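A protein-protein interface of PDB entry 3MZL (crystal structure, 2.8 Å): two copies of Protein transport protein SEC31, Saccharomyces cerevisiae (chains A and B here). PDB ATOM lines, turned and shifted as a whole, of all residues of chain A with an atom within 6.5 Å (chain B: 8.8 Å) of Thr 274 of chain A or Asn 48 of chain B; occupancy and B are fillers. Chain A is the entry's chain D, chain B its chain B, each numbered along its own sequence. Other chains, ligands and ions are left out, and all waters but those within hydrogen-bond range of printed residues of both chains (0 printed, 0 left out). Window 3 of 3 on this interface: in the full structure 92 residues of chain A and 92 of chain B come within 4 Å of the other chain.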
ATOM      1  N   HIS A 269       5.302 -26.898 -27.083  1.00  0.00           N
ATOM      2  CA  HIS A 269       4.123 -26.224 -27.623  1.00  0.00           C
ATOM      3  C   HIS A 269       3.876 -24.878 -26.940  1.00  0.00           C
ATOM      4  O   HIS A 269       3.716 -23.856 -27.612  1.00  0.00           O
ATOM      5  CB  HIS A 269       2.890 -27.125 -27.488  1.00  0.00           C
ATOM      6  CG  HIS A 269       1.601 -26.446 -27.832  1.00  0.00           C
ATOM      7  ND1 HIS A 269       1.203 -26.220 -29.132  1.00  0.00           N
ATOM      8  CD2 HIS A 269       0.618 -25.948 -27.044  1.00  0.00           C
ATOM      9  CE1 HIS A 269       0.032 -25.609 -29.131  1.00  0.00           C
ATOM     10  NE2 HIS A 269      -0.345 -25.431 -27.877  1.00  0.00           N
ATOM     11  N   SER A 270       3.862 -24.893 -25.607  1.00  0.00           N
ATOM     12  CA  SER A 270       3.542 -23.720 -24.793  1.00  0.00           C
ATOM     13  C   SER A 270       4.535 -22.568 -24.973  1.00  0.00           C
ATOM     14  O   SER A 270       4.202 -21.415 -24.695  1.00  0.00           O
ATOM     15  CB  SER A 270       3.449 -24.115 -23.316  1.00  0.00           C
ATOM     16  OG  SER A 270       2.648 -23.201 -22.582  1.00  0.00           O
ATOM     17  N   GLU A 271       5.742 -22.882 -25.439  1.00  0.00           N
ATOM     18  CA  GLU A 271       6.770 -21.867 -25.672  1.00  0.00           C
ATOM     19  C   GLU A 271       6.841 -21.444 -27.139  1.00  0.00           C
ATOM     20  O   GLU A 271       7.122 -20.286 -27.438  1.00  0.00           O
ATOM     21  CB  GLU A 271       8.140 -22.359 -25.192  1.00  0.00           C
ATOM     22  CG  GLU A 271       9.164 -21.251 -24.919  1.00  0.00           C
ATOM     23  CD  GLU A 271       8.821 -20.399 -23.697  1.00  0.00           C
ATOM     24  OE1 GLU A 271       9.296 -20.723 -22.588  1.00  0.00           O
ATOM     25  OE2 GLU A 271       8.073 -19.408 -23.841  1.00  0.00           O
ATOM     26  N   CYS A 272       6.579 -22.388 -28.042  1.00  0.00           N
ATOM     27  CA  CYS A 272       6.631 -22.138 -29.485  1.00  0.00           C
ATOM     28  C   CYS A 272       5.458 -21.289 -29.968  1.00  0.00           C
ATOM     29  O   CYS A 272       5.529 -20.677 -31.036  1.00  0.00           O
ATOM     30  CB  CYS A 272       6.672 -23.457 -30.252  1.00  0.00           C
ATOM     31  SG  CYS A 272       6.830 -23.290 -32.032  1.00  0.00           S
ATOM     32  N   LEU A 273       4.380 -21.272 -29.190  1.00  0.00           N
ATOM     33  CA  LEU A 273       3.269 -20.355 -29.425  1.00  0.00           C
ATOM     34  C   LEU A 273       3.617 -18.969 -28.905  1.00  0.00           C
ATOM     35  O   LEU A 273       3.450 -17.981 -29.612  1.00  0.00           O
ATOM     36  CB  LEU A 273       1.991 -20.850 -28.743  1.00  0.00           C
ATOM     37  CG  LEU A 273       0.960 -21.640 -29.542  1.00  0.00           C
ATOM     38  CD1 LEU A 273      -0.152 -22.075 -28.602  1.00  0.00           C
ATOM     39  CD2 LEU A 273       0.391 -20.827 -30.700  1.00  0.00           C
ATOM     40  N   THR A 274       4.093 -18.916 -27.660  1.00  0.00           N
ATOM     41  CA  THR A 274       4.490 -17.672 -27.001  1.00  0.00           C
ATOM     42  C   THR A 274       5.584 -16.960 -27.796  1.00  0.00           C
ATOM     43  O   THR A 274       5.500 -15.756 -28.028  1.00  0.00           O
ATOM     44  CB  THR A 274       4.977 -17.935 -25.557  1.00  0.00           C
ATOM     45  OG1 THR A 274       4.025 -18.760 -24.871  1.00  0.00           O
ATOM     46  CG2 THR A 274       5.155 -16.626 -24.790  1.00  0.00           C
ATOM     47  N   GLU A 275       6.594 -17.717 -28.221  1.00  0.00           N
ATOM     48  CA  GLU A 275       7.688 -17.185 -29.026  1.00  0.00           C
ATOM     49  C   GLU A 275       7.175 -16.581 -30.325  1.00  0.00           C
ATOM     50  O   GLU A 275       7.498 -15.436 -30.654  1.00  0.00           O
ATOM     51  CB  GLU A 275       8.716 -18.283 -29.320  1.00  0.00           C
ATOM     52  CG  GLU A 275       9.978 -17.790 -30.021  1.00  0.00           C
ATOM     53  CD  GLU A 275       9.770 -17.599 -31.503  1.00  0.00           C
ATOM     54  OE1 GLU A 275       9.128 -18.476 -32.119  1.00  0.00           O
ATOM     55  OE2 GLU A 275      10.237 -16.573 -32.045  1.00  0.00           O
ATOM     56  N   PHE A 276       6.390 -17.369 -31.058  1.00  0.00           N
ATOM     57  CA  PHE A 276       5.712 -16.922 -32.268  1.00  0.00           C
ATOM     58  C   PHE A 276       4.897 -15.654 -31.999  1.00  0.00           C
ATOM     59  O   PHE A 276       5.086 -14.643 -32.678  1.00  0.00           O
ATOM     60  CB  PHE A 276       4.819 -18.048 -32.799  1.00  0.00           C
ATOM     61  CG  PHE A 276       3.983 -17.671 -33.997  1.00  0.00           C
ATOM     62  CD1 PHE A 276       4.448 -17.907 -35.291  1.00  0.00           C
ATOM     63  CD2 PHE A 276       2.713 -17.121 -33.834  1.00  0.00           C
ATOM     64  CE1 PHE A 276       3.673 -17.577 -36.402  1.00  0.00           C
ATOM     65  CE2 PHE A 276       1.931 -16.788 -34.938  1.00  0.00           C
ATOM     66  CZ  PHE A 276       2.412 -17.015 -36.224  1.00  0.00           C
ATOM     67  N   ILE A 277       4.013 -15.710 -31.001  1.00  0.00           N
ATOM     68  CA  ILE A 277       3.150 -14.580 -30.662  1.00  0.00           C
ATOM     69  C   ILE A 277       3.970 -13.346 -30.299  1.00  0.00           C
ATOM     70  O   ILE A 277       3.777 -12.281 -30.889  1.00  0.00           O
ATOM     71  CB  ILE A 277       2.132 -14.931 -29.541  1.00  0.00           C
ATOM     72  CG1 ILE A 277       1.020 -15.852 -30.074  1.00  0.00           C
ATOM     73  CG2 ILE A 277       1.544 -13.667 -28.904  1.00  0.00           C
ATOM     74  CD1 ILE A 277       0.125 -15.256 -31.155  1.00  0.00           C
ATOM     75  N   GLU A 278       4.895 -13.502 -29.353  1.00  0.00           N
ATOM     76  CA  GLU A 278       5.770 -12.406 -28.931  1.00  0.00           C
ATOM     77  C   GLU A 278       6.407 -11.708 -30.138  1.00  0.00           C
ATOM     78  O   GLU A 278       6.387 -10.479 -30.234  1.00  0.00           O
ATOM     79  CB  GLU A 278       6.842 -12.904 -27.951  1.00  0.00           C
ATOM     80  CG  GLU A 278       6.318 -13.144 -26.528  1.00  0.00           C
ATOM     81  CD  GLU A 278       7.368 -13.710 -25.570  1.00  0.00           C
ATOM     82  OE1 GLU A 278       8.273 -14.456 -26.006  1.00  0.00           O
ATOM     83  OE2 GLU A 278       7.277 -13.412 -24.360  1.00  0.00           O
ATOM     84  N   ARG A 279       6.937 -12.508 -31.062  1.00  0.00           N
ATOM     85  CA  ARG A 279       7.563 -12.013 -32.292  1.00  0.00           C
ATOM     86  C   ARG A 279       6.598 -11.180 -33.143  1.00  0.00           C
ATOM     87  O   ARG A 279       6.836  -9.992 -33.379  1.00  0.00           O
ATOM     88  CB  ARG A 279       8.088 -13.193 -33.108  1.00  0.00           C
ATOM     89  CG  ARG A 279       9.263 -12.869 -34.004  1.00  0.00           C
ATOM     90  CD  ARG A 279       9.387 -13.909 -35.101  1.00  0.00           C
ATOM     91  NE  ARG A 279       9.513 -15.264 -34.569  1.00  0.00           N
ATOM     92  CZ  ARG A 279       9.013 -16.351 -35.152  1.00  0.00           C
ATOM     93  NH1 ARG A 279       8.331 -16.257 -36.294  1.00  0.00           N
ATOM     94  NH2 ARG A 279       9.186 -17.539 -34.592  1.00  0.00           N
ATOM     95  N   PHE A 305      -3.356 -19.454 -28.122  1.00  0.00           N
ATOM     96  CA  PHE A 305      -2.633 -18.585 -27.189  1.00  0.00           C
ATOM     97  C   PHE A 305      -3.574 -17.934 -26.173  1.00  0.00           C
ATOM     98  O   PHE A 305      -3.179 -17.703 -25.030  1.00  0.00           O
ATOM     99  CB  PHE A 305      -1.834 -17.519 -27.955  1.00  0.00           C
ATOM    100  CG  PHE A 305      -0.940 -16.670 -27.085  1.00  0.00           C
ATOM    101  CD1 PHE A 305       0.226 -17.198 -26.526  1.00  0.00           C
ATOM    102  CD2 PHE A 305      -1.252 -15.331 -26.844  1.00  0.00           C
ATOM    103  CE1 PHE A 305       1.061 -16.408 -25.723  1.00  0.00           C
ATOM    104  CE2 PHE A 305      -0.425 -14.531 -26.044  1.00  0.00           C
ATOM    105  CZ  PHE A 305       0.734 -15.071 -25.484  1.00  0.00           C
ATOM    106  N   LEU A 308      -4.063 -20.444 -23.454  1.00  0.00           N
ATOM    107  CA  LEU A 308      -2.892 -20.432 -22.581  1.00  0.00           C
ATOM    108  C   LEU A 308      -2.957 -19.233 -21.646  1.00  0.00           C
ATOM    109  O   LEU A 308      -2.686 -19.354 -20.454  1.00  0.00           O
ATOM    110  CB  LEU A 308      -1.591 -20.397 -23.391  1.00  0.00           C
ATOM    111  CG  LEU A 308      -1.145 -21.633 -24.181  1.00  0.00           C
ATOM    112  CD1 LEU A 308       0.203 -21.359 -24.816  1.00  0.00           C
ATOM    113  CD2 LEU A 308      -1.068 -22.894 -23.318  1.00  0.00           C
ATOM    114  N   THR A 312      -3.450 -19.067 -17.307  1.00  0.00           N
ATOM    115  CA  THR A 312      -2.515 -18.358 -16.433  1.00  0.00           C
ATOM    116  C   THR A 312      -3.254 -17.419 -15.474  1.00  0.00           C
ATOM    117  O   THR A 312      -2.673 -16.948 -14.496  1.00  0.00           O
ATOM    118  CB  THR A 312      -1.480 -17.534 -17.241  1.00  0.00           C
ATOM    119  OG1 THR A 312      -2.133 -16.448 -17.906  1.00  0.00           O
ATOM    120  CG2 THR A 312      -0.758 -18.398 -18.270  1.00  0.00           C
ATOM    121  N   ASN A 314      -4.559 -14.533 -16.362  1.00  0.00           N
ATOM    122  CA  ASN A 314      -4.428 -13.203 -16.946  1.00  0.00           C
ATOM    123  C   ASN A 314      -5.531 -12.894 -17.963  1.00  0.00           C
ATOM    124  O   ASN A 314      -5.325 -13.006 -19.174  1.00  0.00           O
ATOM    125  CB  ASN A 314      -3.038 -13.080 -17.590  1.00  0.00           C
ATOM    126  CG  ASN A 314      -2.661 -11.647 -17.946  1.00  0.00           C
ATOM    127  OD1 ASN A 314      -3.414 -10.703 -17.705  1.00  0.00           O
ATOM    128  ND2 ASN A 314      -1.480 -11.486 -18.524  1.00  0.00           N
ATOM    129  N   LEU A 317      -4.872  -9.589 -20.482  1.00  0.00           N
ATOM    130  CA  LEU A 317      -4.107  -9.802 -21.709  1.00  0.00           C
ATOM    131  C   LEU A 317      -4.951 -10.522 -22.754  1.00  0.00           C
ATOM    132  O   LEU A 317      -4.905 -10.184 -23.936  1.00  0.00           O
ATOM    133  CB  LEU A 317      -2.831 -10.600 -21.412  1.00  0.00           C
ATOM    134  CG  LEU A 317      -1.833 -10.908 -22.532  1.00  0.00           C
ATOM    135  CD1 LEU A 317      -1.164  -9.639 -23.030  1.00  0.00           C
ATOM    136  CD2 LEU A 317      -0.786 -11.902 -22.054  1.00  0.00           C
ATOM    137  N   LYS B  41      -0.429 -21.418  -8.572  1.00  0.00           N
ATOM    138  CA  LYS B  41       0.702 -21.043  -9.413  1.00  0.00           C
ATOM    139  C   LYS B  41       1.373 -22.312  -9.924  1.00  0.00           C
ATOM    140  O   LYS B  41       1.935 -23.085  -9.144  1.00  0.00           O
ATOM    141  CB  LYS B  41       1.691 -20.184  -8.614  1.00  0.00           C
ATOM    142  CG  LYS B  41       3.014 -19.863  -9.315  1.00  0.00           C
ATOM    143  CD  LYS B  41       2.857 -18.760 -10.351  1.00  0.00           C
ATOM    144  CE  LYS B  41       4.113 -18.622 -11.194  1.00  0.00           C
ATOM    145  NZ  LYS B  41       3.967 -17.553 -12.218  1.00  0.00           N
ATOM    146  N   GLY B  44       6.390 -23.526 -14.513  1.00  0.00           N
ATOM    147  CA  GLY B  44       6.574 -23.441 -15.966  1.00  0.00           C
ATOM    148  C   GLY B  44       5.354 -22.907 -16.696  1.00  0.00           C
ATOM    149  O   GLY B  44       5.260 -23.002 -17.921  1.00  0.00           O
ATOM    150  N   LEU B  45       4.418 -22.348 -15.932  1.00  0.00           N
ATOM    151  CA  LEU B  45       3.191 -21.772 -16.473  1.00  0.00           C
ATOM    152  C   LEU B  45       2.910 -20.448 -15.759  1.00  0.00           C
ATOM    153  O   LEU B  45       2.248 -20.409 -14.718  1.00  0.00           O
ATOM    154  CB  LEU B  45       2.024 -22.755 -16.320  1.00  0.00           C
ATOM    155  CG  LEU B  45       0.718 -22.517 -17.085  1.00  0.00           C
ATOM    156  CD1 LEU B  45       0.105 -23.843 -17.518  1.00  0.00           C
ATOM    157  CD2 LEU B  45      -0.275 -21.703 -16.262  1.00  0.00           C
ATOM    158  N   GLU B  46       3.434 -19.367 -16.331  1.00  0.00           N
ATOM    159  CA  GLU B  46       3.378 -18.050 -15.710  1.00  0.00           C
ATOM    160  C   GLU B  46       2.489 -17.103 -16.510  1.00  0.00           C
ATOM    161  O   GLU B  46       2.341 -17.260 -17.723  1.00  0.00           O
ATOM    162  CB  GLU B  46       4.790 -17.456 -15.614  1.00  0.00           C
ATOM    163  CG  GLU B  46       5.853 -18.388 -15.024  1.00  0.00           C
ATOM    164  CD  GLU B  46       7.273 -18.047 -15.478  1.00  0.00           C
ATOM    165  OE1 GLU B  46       8.090 -18.982 -15.626  1.00  0.00           O
ATOM    166  OE2 GLU B  46       7.574 -16.851 -15.694  1.00  0.00           O
ATOM    167  N   SER B  47       1.897 -16.126 -15.825  1.00  0.00           N
ATOM    168  CA  SER B  47       1.262 -14.999 -16.497  1.00  0.00           C
ATOM    169  C   SER B  47       2.358 -14.201 -17.194  1.00  0.00           C
ATOM    170  O   SER B  47       3.367 -13.851 -16.577  1.00  0.00           O
ATOM    171  CB  SER B  47       0.526 -14.108 -15.495  1.00  0.00           C
ATOM    172  OG  SER B  47      -0.434 -14.842 -14.754  1.00  0.00           O
ATOM    173  N   ASN B  48       2.169 -13.931 -18.483  1.00  0.00           N
ATOM    174  CA  ASN B  48       3.164 -13.190 -19.256  1.00  0.00           C
ATOM    175  C   ASN B  48       3.226 -11.720 -18.833  1.00  0.00           C
ATOM    176  O   ASN B  48       2.500 -10.873 -19.360  1.00  0.00           O
ATOM    177  CB  ASN B  48       2.897 -13.327 -20.760  1.00  0.00           C
ATOM    178  CG  ASN B  48       4.168 -13.258 -21.590  1.00  0.00           C
ATOM    179  OD1 ASN B  48       5.091 -12.499 -21.282  1.00  0.00           O
ATOM    180  ND2 ASN B  48       4.219 -14.048 -22.654  1.00  0.00           N
ATOM    181  N   THR B  49       4.095 -11.441 -17.862  1.00  0.00           N
ATOM    182  CA  THR B  49       4.271 -10.098 -17.308  1.00  0.00           C
ATOM    183  C   THR B  49       4.854  -9.131 -18.341  1.00  0.00           C
ATOM    184  O   THR B  49       4.322  -8.036 -18.543  1.00  0.00           O
ATOM    185  CB  THR B  49       5.203 -10.121 -16.078  1.00  0.00           C
ATOM    186  OG1 THR B  49       4.944 -11.295 -15.299  1.00  0.00           O
ATOM    187  CG2 THR B  49       4.997  -8.880 -15.218  1.00  0.00           C
ATOM    188  N   THR B  50       5.945  -9.553 -18.984  1.00  0.00           N
ATOM    189  CA  THR B  50       6.653  -8.742 -19.971  1.00  0.00           C
ATOM    190  C   THR B  50       5.756  -8.339 -21.140  1.00  0.00           C
ATOM    191  O   THR B  50       5.731  -7.167 -21.524  1.00  0.00           O
ATOM    192  CB  THR B  50       7.919  -9.455 -20.511  1.00  0.00           C
ATOM    193  OG1 THR B  50       7.592 -10.796 -20.896  1.00  0.00           O
ATOM    194  CG2 THR B  50       9.015  -9.488 -19.455  1.00  0.00           C
ATOM    195  N   LEU B  51       5.013  -9.302 -21.687  1.00  0.00           N
ATOM    196  CA  LEU B  51       4.158  -9.046 -22.850  1.00  0.00           C
ATOM    197  C   LEU B  51       3.024  -8.080 -22.523  1.00  0.00           C
ATOM    198  O   LEU B  51       2.853  -7.074 -23.211  1.00  0.00           O
ATOM    199  CB  LEU B  51       3.612 -10.350 -23.443  1.00  0.00           C
ATOM    200  CG  LEU B  51       2.760 -10.272 -24.717  1.00  0.00           C
ATOM    201  CD1 LEU B  51       3.565  -9.766 -25.918  1.00  0.00           C
ATOM    202  CD2 LEU B  51       2.144 -11.628 -25.019  1.00  0.00           C
ATOM    203  N   SER B  52       2.265  -8.383 -21.472  1.00  0.00           N
ATOM    204  CA  SER B  52       1.166  -7.525 -21.024  1.00  0.00           C
ATOM    205  C   SER B  52       1.641  -6.091 -20.801  1.00  0.00           C
ATOM    206  O   SER B  52       0.911  -5.136 -21.072  1.00  0.00           O
ATOM    207  CB  SER B  52       0.545  -8.076 -19.736  1.00  0.00           C
ATOM    208  OG  SER B  52       0.170  -9.434 -19.894  1.00  0.00           O
ATOM    209  N   GLU B  53       2.875  -5.964 -20.315  1.00  0.00           N
ATOM    210  CA  GLU B  53       3.500  -4.672 -20.058  1.00  0.00           C
ATOM    211  C   GLU B  53       3.889  -3.996 -21.369  1.00  0.00           C
ATOM    212  O   GLU B  53       3.688  -2.794 -21.539  1.00  0.00           O
ATOM    213  CB  GLU B  53       4.733  -4.857 -19.169  1.00  0.00           C
ATOM    214  CG  GLU B  53       5.072  -3.659 -18.297  1.00  0.00           C
ATOM    215  CD  GLU B  53       5.846  -4.042 -17.045  1.00  0.00           C
ATOM    216  OE1 GLU B  53       6.824  -4.819 -17.142  1.00  0.00           O
ATOM    217  OE2 GLU B  53       5.474  -3.557 -15.956  1.00  0.00           O
ATOM    218  N   ALA B  54       4.434  -4.783 -22.291  1.00  0.00           N
ATOM    219  CA  ALA B  54       4.860  -4.287 -23.597  1.00  0.00           C
ATOM    220  C   ALA B  54       3.673  -3.915 -24.487  1.00  0.00           C
ATOM    221  O   ALA B  54       3.823  -3.162 -25.450  1.00  0.00           O
ATOM    222  CB  ALA B  54       5.747  -5.318 -24.291  1.00  0.00           C
ATOM    223  N   LEU B  55       2.498  -4.444 -24.157  1.00  0.00           N
ATOM    224  CA  LEU B  55       1.288  -4.210 -24.939  1.00  0.00           C
ATOM    225  C   LEU B  55       0.520  -2.978 -24.459  1.00  0.00           C
ATOM    226  O   LEU B  55      -0.307  -2.435 -25.193  1.00  0.00           O
ATOM    227  CB  LEU B  55       0.392  -5.455 -24.919  1.00  0.00           C
ATOM    228  CG  LEU B  55      -0.635  -5.666 -26.040  1.00  0.00           C
ATOM    229  CD1 LEU B  55       0.028  -5.758 -27.411  1.00  0.00           C
ATOM    230  CD2 LEU B  55      -1.460  -6.914 -25.766  1.00  0.00           C
ATOM    231  N   LEU B  63      11.328  -7.216 -23.776  1.00  0.00           N
ATOM    232  CA  LEU B  63      10.967  -8.458 -24.464  1.00  0.00           C
ATOM    233  C   LEU B  63      12.087  -8.911 -25.400  1.00  0.00           C
ATOM    234  O   LEU B  63      12.428 -10.096 -25.438  1.00  0.00           O
ATOM    235  CB  LEU B  63       9.661  -8.265 -25.248  1.00  0.00           C
ATOM    236  CG  LEU B  63       8.759  -9.456 -25.603  1.00  0.00           C
ATOM    237  CD1 LEU B  63       7.356  -8.965 -25.931  1.00  0.00           C
ATOM    238  CD2 LEU B  63       9.306 -10.288 -26.757  1.00  0.00           C
ATOM    239  N   GLN B  66      14.847 -10.602 -23.674  1.00  0.00           N
ATOM    240  CA  GLN B  66      14.479 -11.968 -23.318  1.00  0.00           C
ATOM    241  C   GLN B  66      14.659 -12.918 -24.502  1.00  0.00           C
ATOM    242  O   GLN B  66      15.394 -13.902 -24.404  1.00  0.00           O
ATOM    243  CB  GLN B  66      13.044 -12.039 -22.785  1.00  0.00           C
ATOM    244  CG  GLN B  66      12.861 -11.445 -21.402  1.00  0.00           C
ATOM    245  CD  GLN B  66      11.893 -12.241 -20.538  1.00  0.00           C
ATOM    246  OE1 GLN B  66      10.833 -12.682 -20.998  1.00  0.00           O
ATOM    247  NE2 GLN B  66      12.253 -12.423 -19.273  1.00  0.00           N
ATOM    248  N   ARG B  67      14.013 -12.605 -25.622  1.00  0.00           N
ATOM    249  CA  ARG B  67      14.001 -13.501 -26.783  1.00  0.00           C
ATOM    250  C   ARG B  67      15.311 -13.531 -27.587  1.00  0.00           C
ATOM    251  O   ARG B  67      15.502 -14.405 -28.440  1.00  0.00           O
ATOM    252  CB  ARG B  67      12.795 -13.197 -27.686  1.00  0.00           C
ATOM    253  CG  ARG B  67      11.465 -13.793 -27.191  1.00  0.00           C
ATOM    254  CD  ARG B  67      11.375 -15.289 -27.499  1.00  0.00           C
ATOM    255  NE  ARG B  67      10.236 -15.931 -26.843  1.00  0.00           N
ATOM    256  CZ  ARG B  67      10.151 -17.233 -26.566  1.00  0.00           C
ATOM    257  NH1 ARG B  67      11.137 -18.062 -26.890  1.00  0.00           N
ATOM    258  NH2 ARG B  67       9.068 -17.713 -25.969  1.00  0.00           N
ATOM    259  N   TRP B  80      14.659 -11.810 -34.925  1.00  0.00           N
ATOM    260  CA  TRP B  80      14.749 -11.029 -33.693  1.00  0.00           C
ATOM    261  C   TRP B  80      15.764  -9.892 -33.808  1.00  0.00           C
ATOM    262  O   TRP B  80      15.500  -8.778 -33.350  1.00  0.00           O
ATOM    263  CB  TRP B  80      15.023 -11.927 -32.481  1.00  0.00           C
ATOM    264  CG  TRP B  80      13.814 -12.729 -32.062  1.00  0.00           C
ATOM    265  CD1 TRP B  80      13.588 -14.061 -32.289  1.00  0.00           C
ATOM    266  CD2 TRP B  80      12.661 -12.245 -31.362  1.00  0.00           C
ATOM    267  NE1 TRP B  80      12.371 -14.434 -31.769  1.00  0.00           N
ATOM    268  CE2 TRP B  80      11.783 -13.339 -31.193  1.00  0.00           C
ATOM    269  CE3 TRP B  80      12.287 -10.991 -30.856  1.00  0.00           C
ATOM    270  CZ2 TRP B  80      10.552 -13.217 -30.542  1.00  0.00           C
ATOM    271  CZ3 TRP B  80      11.059 -10.873 -30.207  1.00  0.00           C
ATOM    272  CH2 TRP B  80      10.211 -11.980 -30.055  1.00  0.00           C
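No position is printed for both chains.
Among the printed residues, merely in contact across the chains: Thr 274 of chain A with Asn 48 of chain B, Glu 278 of chain A with Asn 48 of chain B, Glu 278 of chain A with Leu 63 of chain B, Glu 278 of chain A with Trp 80 of chain B, Arg 279 of chain A with Trp 80 of chain B, Phe 305 of chain A with Leu 51 of chain B, Thr 312 of chain A with Leu 45 of chain B, Thr 312 of chain A with Glu 46 of chain B, Leu 317 of chain A with Ser 52 of chain B and Leu 317 of chain A with Leu 55 of chain B.
Asn 48 of chain B touches just these residues of chain A: Thr 274 (3.5 Å) and Glu 278 (3.6 Å). Printed residues of chain B within 4 Å of Glu 275 of chain A: Arg 67 (3.3 Å) and Trp 80 (3.0 Å). Printed residues of chain A within 4 Å of Ser 52 of chain B: Asn 314 and Leu 317. Of the printed residues of chain A, Trp 80 of chain B touches Glu 275, Glu 278 and Arg 279. The nearest printed residue of chain B that does not touch Thr 274 of chain A is Arg 67 of chain B (4.01 Å). The nearest printed residue of chain B that does not touch Arg 279 of chain A is Leu 63 of chain B (5.4 Å).
O of Ser 47 of chain B lies within hydrogen-bond range of OG1 of Thr 49 of chain B, 3.3 Å away. The side-chain amide oxygen (OD1) of Asn 48 of chain B is in hydrogen-bond range of the backbone NH (N) of Leu 51 of chain B (3.2 Å). The backbone carbonyl oxygen of Ser 270 of chain A sits at hydrogen-bond distance from the side-chain hydroxyl of Thr 274 of chain A, 2.7 Å away. The guanidinium group (NH2) of Arg 279 of chain A is in salt-bridge range of the side-chain carboxylate (OE1) of Glu 275 of chain A, 2.6 Å away. N of Asn 314 of chain A sits close to OG1 of Thr 312 of chain A. The side-chain amide oxygen (OD1) of Asn 314 of chain A is in hydrogen-bond range of the backbone NH (N) of Leu 317 of chain A, at 3.3 Å.
Of the 16 printed residues of chain A, 9 touch a printed residue of chain B. Printed residues of chain A that touch a printed residue of chain B: Glu 271, Thr 274, Glu 275, Glu 278, Arg 279, Phe 305, Thr 312, Asn 314 and Leu 317. Hydrophobic or aromatic side chains of chain A within 4 Å of the printed part of chain B: Phe 305 and Leu 317. Printed residues of chain B that touch a printed residue of chain A: Leu 45, Glu 46, Ser 47, Asn 48, Leu 51, Ser 52, Leu 55, Leu 63, Arg 67 and Trp 80. Among the printed residues, 16 pairs touch across the chains. Among the printed residues, Asp or Glu carboxylates within 4 Å of a Lys or Arg side-chain nitrogen of the other chain: Glu 271 of chain A with Arg 67 of chain B and Glu 278 of chain A with Arg 67 of chain B.
The side-chain hydroxyl (OG) of Ser 47 of chain B sits at hydrogen-bond distance from the backbone carbonyl oxygen (O) of Thr 312 of chain A (3.1 Å). The side-chain hydroxyl (OG) of Ser 52 of chain B lies within hydrogen-bond range of the side-chain amide nitrogen (ND2) of Asn 314 of chain A (3.0 Å). NH2 of Arg 67 of chain B lies within salt-bridge range of OE2 of Glu 271 of chain A, at 2.9 Å. OE1 of Glu 278 of chain A is in salt-bridge range of NE of Arg 67 of chain B, at 2.6 Å. NE1 of Trp 80 of chain B is in hydrogen-bond range of OE2 of Glu 275 of chain A (3.0 Å). The backbone NH (N) of Glu 275 of chain A lies close to the guanidinium group (NH2) of Arg 67 of chain B, 3.3 Å away.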
